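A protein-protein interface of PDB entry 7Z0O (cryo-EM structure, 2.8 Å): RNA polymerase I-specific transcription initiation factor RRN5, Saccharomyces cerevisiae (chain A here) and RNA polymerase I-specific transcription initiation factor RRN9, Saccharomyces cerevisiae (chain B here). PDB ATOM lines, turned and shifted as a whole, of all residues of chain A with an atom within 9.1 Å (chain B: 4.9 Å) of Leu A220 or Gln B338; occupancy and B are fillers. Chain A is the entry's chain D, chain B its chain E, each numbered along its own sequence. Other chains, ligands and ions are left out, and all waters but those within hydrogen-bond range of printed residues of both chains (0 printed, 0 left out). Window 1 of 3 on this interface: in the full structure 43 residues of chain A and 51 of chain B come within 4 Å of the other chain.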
ATOM      1  N   THR A 211      21.796   1.239 -26.000  1.00  0.00           N
ATOM      2  CA  THR A 211      22.716   0.391 -25.250  1.00  0.00           C
ATOM      3  C   THR A 211      22.456   0.499 -23.755  1.00  0.00           C
ATOM      4  O   THR A 211      22.524  -0.500 -23.030  1.00  0.00           O
ATOM      5  CB  THR A 211      24.159   0.766 -25.576  1.00  0.00           C
ATOM      6  OG1 THR A 211      24.371   0.647 -26.986  1.00  0.00           O
ATOM      7  CG2 THR A 211      25.127  -0.151 -24.852  1.00  0.00           C
ATOM      8  N   ARG A 212      22.156   1.706 -23.274  1.00  0.00           N
ATOM      9  CA  ARG A 212      21.741   1.866 -21.886  1.00  0.00           C
ATOM     10  C   ARG A 212      20.452   1.103 -21.614  1.00  0.00           C
ATOM     11  O   ARG A 212      20.319   0.433 -20.587  1.00  0.00           O
ATOM     12  CB  ARG A 212      21.569   3.347 -21.560  1.00  0.00           C
ATOM     13  CG  ARG A 212      22.871   4.099 -21.401  1.00  0.00           C
ATOM     14  CD  ARG A 212      22.631   5.480 -20.830  1.00  0.00           C
ATOM     15  NE  ARG A 212      23.010   5.556 -19.425  1.00  0.00           N
ATOM     16  CZ  ARG A 212      24.246   5.764 -18.996  1.00  0.00           C
ATOM     17  NH1 ARG A 212      25.252   5.928 -19.839  1.00  0.00           N
ATOM     18  NH2 ARG A 212      24.480   5.807 -17.688  1.00  0.00           N
ATOM     19  N   THR A 213      19.490   1.190 -22.533  1.00  0.00           N
ATOM     20  CA  THR A 213      18.243   0.451 -22.366  1.00  0.00           C
ATOM     21  C   THR A 213      18.494  -1.049 -22.323  1.00  0.00           C
ATOM     22  O   THR A 213      17.914  -1.761 -21.496  1.00  0.00           O
ATOM     23  CB  THR A 213      17.274   0.796 -23.495  1.00  0.00           C
ATOM     24  OG1 THR A 213      17.072   2.213 -23.538  1.00  0.00           O
ATOM     25  CG2 THR A 213      15.941   0.105 -23.283  1.00  0.00           C
ATOM     26  N   LEU A 214      19.357  -1.547 -23.209  1.00  0.00           N
ATOM     27  CA  LEU A 214      19.666  -2.972 -23.227  1.00  0.00           C
ATOM     28  C   LEU A 214      20.379  -3.406 -21.953  1.00  0.00           C
ATOM     29  O   LEU A 214      20.045  -4.444 -21.371  1.00  0.00           O
ATOM     30  CB  LEU A 214      20.517  -3.299 -24.451  1.00  0.00           C
ATOM     31  CG  LEU A 214      20.781  -4.775 -24.722  1.00  0.00           C
ATOM     32  CD1 LEU A 214      19.485  -5.557 -24.703  1.00  0.00           C
ATOM     33  CD2 LEU A 214      21.487  -4.934 -26.049  1.00  0.00           C
ATOM     34  N   LEU A 215      21.365  -2.627 -21.507  1.00  0.00           N
ATOM     35  CA  LEU A 215      22.128  -3.000 -20.320  1.00  0.00           C
ATOM     36  C   LEU A 215      21.250  -2.997 -19.077  1.00  0.00           C
ATOM     37  O   LEU A 215      21.395  -3.856 -18.199  1.00  0.00           O
ATOM     38  CB  LEU A 215      23.315  -2.057 -20.140  1.00  0.00           C
ATOM     39  CG  LEU A 215      24.557  -2.376 -20.971  1.00  0.00           C
ATOM     40  CD1 LEU A 215      25.779  -1.707 -20.377  1.00  0.00           C
ATOM     41  CD2 LEU A 215      24.759  -3.875 -21.065  1.00  0.00           C
ATOM     42  N   TRP A 216      20.336  -2.035 -18.982  1.00  0.00           N
ATOM     43  CA  TRP A 216      19.447  -1.959 -17.832  1.00  0.00           C
ATOM     44  C   TRP A 216      18.374  -3.035 -17.850  1.00  0.00           C
ATOM     45  O   TRP A 216      17.657  -3.188 -16.856  1.00  0.00           O
ATOM     46  CB  TRP A 216      18.815  -0.570 -17.769  1.00  0.00           C
ATOM     47  CG  TRP A 216      19.781   0.478 -17.325  1.00  0.00           C
ATOM     48  CD1 TRP A 216      21.028   0.712 -17.827  1.00  0.00           C
ATOM     49  CD2 TRP A 216      19.592   1.422 -16.274  1.00  0.00           C
ATOM     50  NE1 TRP A 216      21.622   1.751 -17.160  1.00  0.00           N
ATOM     51  CE2 TRP A 216      20.759   2.205 -16.199  1.00  0.00           C
ATOM     52  CE3 TRP A 216      18.546   1.686 -15.392  1.00  0.00           C
ATOM     53  CZ2 TRP A 216      20.909   3.229 -15.276  1.00  0.00           C
ATOM     54  CZ3 TRP A 216      18.696   2.700 -14.482  1.00  0.00           C
ATOM     55  CH2 TRP A 216      19.868   3.461 -14.427  1.00  0.00           C
ATOM     56  N   CYS A 217      18.242  -3.780 -18.945  1.00  0.00           N
ATOM     57  CA  CYS A 217      17.289  -4.878 -19.009  1.00  0.00           C
ATOM     58  C   CYS A 217      17.952  -6.230 -18.782  1.00  0.00           C
ATOM     59  O   CYS A 217      17.281  -7.186 -18.382  1.00  0.00           O
ATOM     60  CB  CYS A 217      16.570  -4.874 -20.359  1.00  0.00           C
ATOM     61  SG  CYS A 217      14.941  -4.106 -20.329  1.00  0.00           S
ATOM     62  N   THR A 218      19.256  -6.334 -19.036  1.00  0.00           N
ATOM     63  CA  THR A 218      19.983  -7.586 -18.877  1.00  0.00           C
ATOM     64  C   THR A 218      21.030  -7.509 -17.773  1.00  0.00           C
ATOM     65  O   THR A 218      20.996  -8.304 -16.831  1.00  0.00           O
ATOM     66  CB  THR A 218      20.647  -7.982 -20.204  1.00  0.00           C
ATOM     67  OG1 THR A 218      21.806  -7.170 -20.421  1.00  0.00           O
ATOM     68  CG2 THR A 218      19.686  -7.793 -21.362  1.00  0.00           C
ATOM     69  N   ALA A 219      21.962  -6.560 -17.863  1.00  0.00           N
ATOM     70  CA  ALA A 219      23.045  -6.473 -16.892  1.00  0.00           C
ATOM     71  C   ALA A 219      22.578  -6.010 -15.521  1.00  0.00           C
ATOM     72  O   ALA A 219      23.016  -6.572 -14.512  1.00  0.00           O
ATOM     73  CB  ALA A 219      24.138  -5.535 -17.404  1.00  0.00           C
ATOM     74  N   LEU A 220      21.711  -5.003 -15.456  1.00  0.00           N
ATOM     75  CA  LEU A 220      21.205  -4.523 -14.177  1.00  0.00           C
ATOM     76  C   LEU A 220      20.155  -5.445 -13.578  1.00  0.00           C
ATOM     77  O   LEU A 220      20.028  -5.511 -12.352  1.00  0.00           O
ATOM     78  CB  LEU A 220      20.623  -3.117 -14.334  1.00  0.00           C
ATOM     79  CG  LEU A 220      20.301  -2.359 -13.045  1.00  0.00           C
ATOM     80  CD1 LEU A 220      21.575  -1.985 -12.315  1.00  0.00           C
ATOM     81  CD2 LEU A 220      19.483  -1.125 -13.348  1.00  0.00           C
ATOM     82  N   ALA A 221      19.400  -6.159 -14.414  1.00  0.00           N
ATOM     83  CA  ALA A 221      18.376  -7.061 -13.898  1.00  0.00           C
ATOM     84  C   ALA A 221      18.992  -8.196 -13.089  1.00  0.00           C
ATOM     85  O   ALA A 221      18.464  -8.577 -12.038  1.00  0.00           O
ATOM     86  CB  ALA A 221      17.536  -7.612 -15.047  1.00  0.00           C
ATOM     87  N   GLY A 222      20.111  -8.744 -13.558  1.00  0.00           N
ATOM     88  CA  GLY A 222      20.769  -9.839 -12.871  1.00  0.00           C
ATOM     89  C   GLY A 222      21.843  -9.380 -11.907  1.00  0.00           C
ATOM     90  O   GLY A 222      22.713 -10.161 -11.516  1.00  0.00           O
ATOM     91  N   MET A 223      21.786  -8.105 -11.523  1.00  0.00           N
ATOM     92  CA  MET A 223      22.769  -7.545 -10.601  1.00  0.00           C
ATOM     93  C   MET A 223      22.792  -8.282  -9.268  1.00  0.00           C
ATOM     94  O   MET A 223      23.833  -8.326  -8.603  1.00  0.00           O
ATOM     95  CB  MET A 223      22.466  -6.065 -10.374  1.00  0.00           C
ATOM     96  CG  MET A 223      23.671  -5.158 -10.266  1.00  0.00           C
ATOM     97  SD  MET A 223      23.185  -3.607  -9.489  1.00  0.00           S
ATOM     98  CE  MET A 223      24.753  -3.005  -8.887  1.00  0.00           C
ATOM     99  N   ALA A 224      21.664  -8.861  -8.859  1.00  0.00           N
ATOM    100  CA  ALA A 224      21.569  -9.501  -7.554  1.00  0.00           C
ATOM    101  C   ALA A 224      22.007 -10.960  -7.562  1.00  0.00           C
ATOM    102  O   ALA A 224      22.072 -11.571  -6.491  1.00  0.00           O
ATOM    103  CB  ALA A 224      20.137  -9.404  -7.027  1.00  0.00           C
ATOM    104  N   SER A 225      22.301 -11.534  -8.726  1.00  0.00           N
ATOM    105  CA  SER A 225      22.739 -12.926  -8.818  1.00  0.00           C
ATOM    106  C   SER A 225      24.260 -12.943  -8.892  1.00  0.00           C
ATOM    107  O   SER A 225      24.845 -12.681  -9.944  1.00  0.00           O
ATOM    108  CB  SER A 225      22.113 -13.609 -10.027  1.00  0.00           C
ATOM    109  OG  SER A 225      20.763 -13.954  -9.771  1.00  0.00           O
ATOM    110  N   ARG A 226      24.902 -13.261  -7.775  1.00  0.00           N
ATOM    111  CA  ARG A 226      26.353 -13.250  -7.691  1.00  0.00           C
ATOM    112  C   ARG A 226      26.928 -14.615  -8.047  1.00  0.00           C
ATOM    113  O   ARG A 226      26.227 -15.626  -8.078  1.00  0.00           O
ATOM    114  CB  ARG A 226      26.809 -12.840  -6.292  1.00  0.00           C
ATOM    115  CG  ARG A 226      26.048 -11.665  -5.715  1.00  0.00           C
ATOM    116  CD  ARG A 226      26.205 -10.436  -6.585  1.00  0.00           C
ATOM    117  NE  ARG A 226      27.448  -9.727  -6.306  1.00  0.00           N
ATOM    118  CZ  ARG A 226      27.709  -8.493  -6.712  1.00  0.00           C
ATOM    119  NH1 ARG A 226      26.834  -7.799  -7.421  1.00  0.00           N
ATOM    120  NH2 ARG A 226      28.878  -7.941  -6.400  1.00  0.00           N
ATOM    121  N   THR A 243      29.352 -10.218 -10.167  1.00  0.00           N
ATOM    122  CA  THR A 243      28.187 -10.479 -10.999  1.00  0.00           C
ATOM    123  C   THR A 243      28.653 -10.707 -12.428  1.00  0.00           C
ATOM    124  O   THR A 243      29.411  -9.898 -12.974  1.00  0.00           O
ATOM    125  CB  THR A 243      27.194  -9.318 -10.947  1.00  0.00           C
ATOM    126  OG1 THR A 243      26.882  -9.015  -9.583  1.00  0.00           O
ATOM    127  CG2 THR A 243      25.921  -9.681 -11.682  1.00  0.00           C
ATOM    128  N   VAL A 245      27.674 -11.596 -16.449  1.00  0.00           N
ATOM    129  CA  VAL A 245      26.688 -11.600 -17.520  1.00  0.00           C
ATOM    130  C   VAL A 245      27.138 -12.605 -18.567  1.00  0.00           C
ATOM    131  O   VAL A 245      28.302 -12.594 -18.985  1.00  0.00           O
ATOM    132  CB  VAL A 245      26.521 -10.200 -18.132  1.00  0.00           C
ATOM    133  CG1 VAL A 245      25.354 -10.182 -19.100  1.00  0.00           C
ATOM    134  CG2 VAL A 245      26.330  -9.168 -17.040  1.00  0.00           C
ATOM    135  N   GLN A 249      22.118 -15.599 -20.315  1.00  0.00           N
ATOM    136  CA  GLN A 249      21.244 -14.643 -19.647  1.00  0.00           C
ATOM    137  C   GLN A 249      20.773 -13.547 -20.590  1.00  0.00           C
ATOM    138  O   GLN A 249      19.646 -13.060 -20.458  1.00  0.00           O
ATOM    139  CB  GLN A 249      21.958 -14.031 -18.444  1.00  0.00           C
ATOM    140  CG  GLN A 249      22.334 -15.034 -17.371  1.00  0.00           C
ATOM    141  CD  GLN A 249      23.419 -14.516 -16.452  1.00  0.00           C
ATOM    142  OE1 GLN A 249      23.597 -13.308 -16.303  1.00  0.00           O
ATOM    143  NE2 GLN A 249      24.153 -15.429 -15.829  1.00  0.00           N
ATOM    144  N   ALA A 253      16.947 -12.874 -21.445  1.00  0.00           N
ATOM    145  CA  ALA A 253      16.342 -11.571 -21.192  1.00  0.00           C
ATOM    146  C   ALA A 253      15.663 -11.021 -22.439  1.00  0.00           C
ATOM    147  O   ALA A 253      14.583 -10.430 -22.351  1.00  0.00           O
ATOM    148  CB  ALA A 253      17.400 -10.593 -20.684  1.00  0.00           C
ATOM    149  N   GLU A 257      11.459 -10.836 -22.027  1.00  0.00           N
ATOM    150  CA  GLU A 257      11.116  -9.504 -21.559  1.00  0.00           C
ATOM    151  C   GLU A 257       9.786  -9.054 -22.155  1.00  0.00           C
ATOM    152  O   GLU A 257       9.292  -9.614 -23.137  1.00  0.00           O
ATOM    153  CB  GLU A 257      12.212  -8.502 -21.916  1.00  0.00           C
ATOM    154  CG  GLU A 257      12.353  -7.358 -20.930  1.00  0.00           C
ATOM    155  CD  GLU A 257      12.803  -7.823 -19.561  1.00  0.00           C
ATOM    156  OE1 GLU A 257      13.586  -8.793 -19.490  1.00  0.00           O
ATOM    157  OE2 GLU A 257      12.373  -7.220 -18.556  1.00  0.00           O
ATOM    158  N   ARG A 261       9.232  -3.270 -23.831  1.00  0.00           N
ATOM    159  CA  ARG A 261      10.617  -2.880 -23.600  1.00  0.00           C
ATOM    160  C   ARG A 261      11.373  -2.632 -24.898  1.00  0.00           C
ATOM    161  O   ARG A 261      12.510  -2.153 -24.849  1.00  0.00           O
ATOM    162  CB  ARG A 261      11.330  -3.952 -22.777  1.00  0.00           C
ATOM    163  CG  ARG A 261      10.849  -4.050 -21.342  1.00  0.00           C
ATOM    164  CD  ARG A 261      11.544  -3.040 -20.449  1.00  0.00           C
ATOM    165  NE  ARG A 261      10.853  -1.758 -20.433  1.00  0.00           N
ATOM    166  CZ  ARG A 261      10.960  -0.861 -19.461  1.00  0.00           C
ATOM    167  NH1 ARG A 261      11.735  -1.072 -18.410  1.00  0.00           N
ATOM    168  NH2 ARG A 261      10.273   0.274 -19.547  1.00  0.00           N
ATOM    169  N   SER B 236      10.771  -2.720  -8.835  1.00  0.00           N
ATOM    170  CA  SER B 236      11.223  -2.929 -10.206  1.00  0.00           C
ATOM    171  C   SER B 236      10.047  -3.135 -11.150  1.00  0.00           C
ATOM    172  O   SER B 236      10.054  -2.633 -12.279  1.00  0.00           O
ATOM    173  CB  SER B 236      12.171  -4.124 -10.268  1.00  0.00           C
ATOM    174  OG  SER B 236      13.312  -3.910  -9.457  1.00  0.00           O
ATOM    175  N   CYS B 239       8.457   0.122 -12.061  1.00  0.00           N
ATOM    176  CA  CYS B 239       9.265   0.843 -13.036  1.00  0.00           C
ATOM    177  C   CYS B 239       9.052   0.293 -14.440  1.00  0.00           C
ATOM    178  O   CYS B 239       9.082   1.043 -15.421  1.00  0.00           O
ATOM    179  CB  CYS B 239      10.741   0.775 -12.648  1.00  0.00           C
ATOM    180  SG  CYS B 239      11.140   1.600 -11.095  1.00  0.00           S
ATOM    181  N   ARG B 334      20.655  -1.996  -7.255  1.00  0.00           N
ATOM    182  CA  ARG B 334      19.884  -2.295  -8.458  1.00  0.00           C
ATOM    183  C   ARG B 334      18.577  -1.513  -8.490  1.00  0.00           C
ATOM    184  O   ARG B 334      18.209  -0.938  -9.520  1.00  0.00           O
ATOM    185  CB  ARG B 334      19.612  -3.794  -8.547  1.00  0.00           C
ATOM    186  CG  ARG B 334      18.728  -4.184  -9.710  1.00  0.00           C
ATOM    187  CD  ARG B 334      18.195  -5.587  -9.542  1.00  0.00           C
ATOM    188  NE  ARG B 334      17.004  -5.618  -8.704  1.00  0.00           N
ATOM    189  CZ  ARG B 334      16.203  -6.667  -8.585  1.00  0.00           C
ATOM    190  NH1 ARG B 334      16.444  -7.795  -9.231  1.00  0.00           N
ATOM    191  NH2 ARG B 334      15.137  -6.583  -7.797  1.00  0.00           N
ATOM    192  N   THR B 335      17.857  -1.482  -7.368  1.00  0.00           N
ATOM    193  CA  THR B 335      16.596  -0.752  -7.332  1.00  0.00           C
ATOM    194  C   THR B 335      16.821   0.751  -7.264  1.00  0.00           C
ATOM    195  O   THR B 335      15.957   1.522  -7.697  1.00  0.00           O
ATOM    196  CB  THR B 335      15.748  -1.215  -6.153  1.00  0.00           C
ATOM    197  OG1 THR B 335      16.452  -0.968  -4.931  1.00  0.00           O
ATOM    198  CG2 THR B 335      15.461  -2.695  -6.272  1.00  0.00           C
ATOM    199  N   PHE B 336      17.957   1.187  -6.719  1.00  0.00           N
ATOM    200  CA  PHE B 336      18.275   2.609  -6.730  1.00  0.00           C
ATOM    201  C   PHE B 336      18.391   3.125  -8.157  1.00  0.00           C
ATOM    202  O   PHE B 336      17.857   4.187  -8.492  1.00  0.00           O
ATOM    203  CB  PHE B 336      19.570   2.867  -5.963  1.00  0.00           C
ATOM    204  CG  PHE B 336      20.149   4.231  -6.199  1.00  0.00           C
ATOM    205  CD1 PHE B 336      19.695   5.322  -5.482  1.00  0.00           C
ATOM    206  CD2 PHE B 336      21.144   4.425  -7.140  1.00  0.00           C
ATOM    207  CE1 PHE B 336      20.222   6.577  -5.697  1.00  0.00           C
ATOM    208  CE2 PHE B 336      21.673   5.678  -7.360  1.00  0.00           C
ATOM    209  CZ  PHE B 336      21.212   6.755  -6.636  1.00  0.00           C
ATOM    210  N   PHE B 337      19.090   2.380  -9.014  1.00  0.00           N
ATOM    211  CA  PHE B 337      19.245   2.814 -10.396  1.00  0.00           C
ATOM    212  C   PHE B 337      17.955   2.651 -11.184  1.00  0.00           C
ATOM    213  O   PHE B 337      17.571   3.560 -11.924  1.00  0.00           O
ATOM    214  CB  PHE B 337      20.390   2.051 -11.059  1.00  0.00           C
ATOM    215  CG  PHE B 337      21.746   2.582 -10.701  1.00  0.00           C
ATOM    216  CD1 PHE B 337      22.241   3.718 -11.313  1.00  0.00           C
ATOM    217  CD2 PHE B 337      22.519   1.957  -9.741  1.00  0.00           C
ATOM    218  CE1 PHE B 337      23.482   4.215 -10.981  1.00  0.00           C
ATOM    219  CE2 PHE B 337      23.762   2.450  -9.404  1.00  0.00           C
ATOM    220  CZ  PHE B 337      24.244   3.579 -10.025  1.00  0.00           C
ATOM    221  N   GLN B 338      17.262   1.520 -11.021  1.00  0.00           N
ATOM    222  CA  GLN B 338      16.010   1.308 -11.741  1.00  0.00           C
ATOM    223  C   GLN B 338      15.006   2.413 -11.441  1.00  0.00           C
ATOM    224  O   GLN B 338      14.265   2.844 -12.331  1.00  0.00           O
ATOM    225  CB  GLN B 338      15.425  -0.057 -11.388  1.00  0.00           C
ATOM    226  CG  GLN B 338      15.984  -1.200 -12.210  1.00  0.00           C
ATOM    227  CD  GLN B 338      15.544  -2.555 -11.696  1.00  0.00           C
ATOM    228  OE1 GLN B 338      15.028  -2.671 -10.587  1.00  0.00           O
ATOM    229  NE2 GLN B 338      15.746  -3.588 -12.504  1.00  0.00           N
ATOM    230  N   VAL B 339      14.965   2.881 -10.194  1.00  0.00           N
ATOM    231  CA  VAL B 339      14.127   4.027  -9.859  1.00  0.00           C
ATOM    232  C   VAL B 339      14.619   5.275 -10.576  1.00  0.00           C
ATOM    233  O   VAL B 339      13.823   6.052 -11.117  1.00  0.00           O
ATOM    234  CB  VAL B 339      14.089   4.223  -8.333  1.00  0.00           C
ATOM    235  CG1 VAL B 339      13.722   5.650  -7.985  1.00  0.00           C
ATOM    236  CG2 VAL B 339      13.107   3.256  -7.709  1.00  0.00           C
ATOM    237  N   LYS B 340      15.937   5.486 -10.600  1.00  0.00           N
ATOM    238  CA  LYS B 340      16.492   6.663 -11.259  1.00  0.00           C
ATOM    239  C   LYS B 340      16.210   6.659 -12.755  1.00  0.00           C
ATOM    240  O   LYS B 340      15.920   7.711 -13.334  1.00  0.00           O
ATOM    241  CB  LYS B 340      17.996   6.746 -11.005  1.00  0.00           C
ATOM    242  CG  LYS B 340      18.607   8.087 -11.363  1.00  0.00           C
ATOM    243  CD  LYS B 340      20.086   8.134 -11.020  1.00  0.00           C
ATOM    244  CE  LYS B 340      20.856   7.046 -11.747  1.00  0.00           C
ATOM    245  NZ  LYS B 340      20.487   6.966 -13.187  1.00  0.00           N
ATOM    246  N   GLY B 341      16.292   5.499 -13.395  1.00  0.00           N
ATOM    247  CA  GLY B 341      16.038   5.395 -14.814  1.00  0.00           C
ATOM    248  C   GLY B 341      17.311   5.468 -15.640  1.00  0.00           C
ATOM    249  O   GLY B 341      18.315   6.058 -15.248  1.00  0.00           O
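No residue of chain A comes within 4 Å of Val B339.
Printed residues of chain B within 4 Å of Ala A221: Arg B334 (3.5 Å).
Of the printed residues of chain A, Gly B341 touches Trp A216.
Printed residues of chain A within 4 Å of Lys B340: Trp A216.
Of the printed residues of chain A, Arg B334 touches Leu A220 (3.2 Å), Ala A221 (3.5 Å) and Met A223 (3.7 Å).
Of the printed residues of chain A, Phe B337 touches Trp A216.
The nearest residue of chain A that does not touch Gln B338 is Ala A221 (4.6 Å).
The nearest printed residue of chain B that does not touch Trp A216 is Val B339 (5.7 Å).
Of the 10 printed residues of chain B, 5 touch a printed residue of chain A.
Along chain B the printed residues that touch a printed residue of chain A span positions 334 to 341.
Hydrophobic or aromatic side chains of chain A that line the printed part of chain B: Trp A216, Leu A220 and Met A223.
The side-chain sulfur of Cys B239 sits at hydrogen-bond distance from the backbone carbonyl oxygen of Gln B338, at 3.6 Å.
The backbone carbonyl oxygen (O) of Met A223 lies within hydrogen-bond range of the guanidinium group (NH1) of Arg A226, at 3.3 Å.
The backbone carbonyl oxygen (O) of Leu A215 sits at hydrogen-bond distance from the backbone NH (N) of Leu A220.
The side-chain hydroxyl (OG1) of Thr A243 lies within hydrogen-bond range of the backbone carbonyl oxygen (O) of Met A223.
The side-chain sulfur of Met A223 lies close to the backbone NH of Arg B334, 3.7 Å away.
Among the printed residues, pairs that only touch across the chains: Trp A216 with Phe B337 (2.9 Å), Trp A216 with Gly B341 (3.1 Å), Leu A220 with Arg B334 (3.2 Å), Ala A221 with Arg B334 (3.5 Å), Leu A220 with Gln B338 (3.7 Å), Trp A216 with Lys B340 (3.8 Å) and Trp A216 with Gln B338 (3.9 Å).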
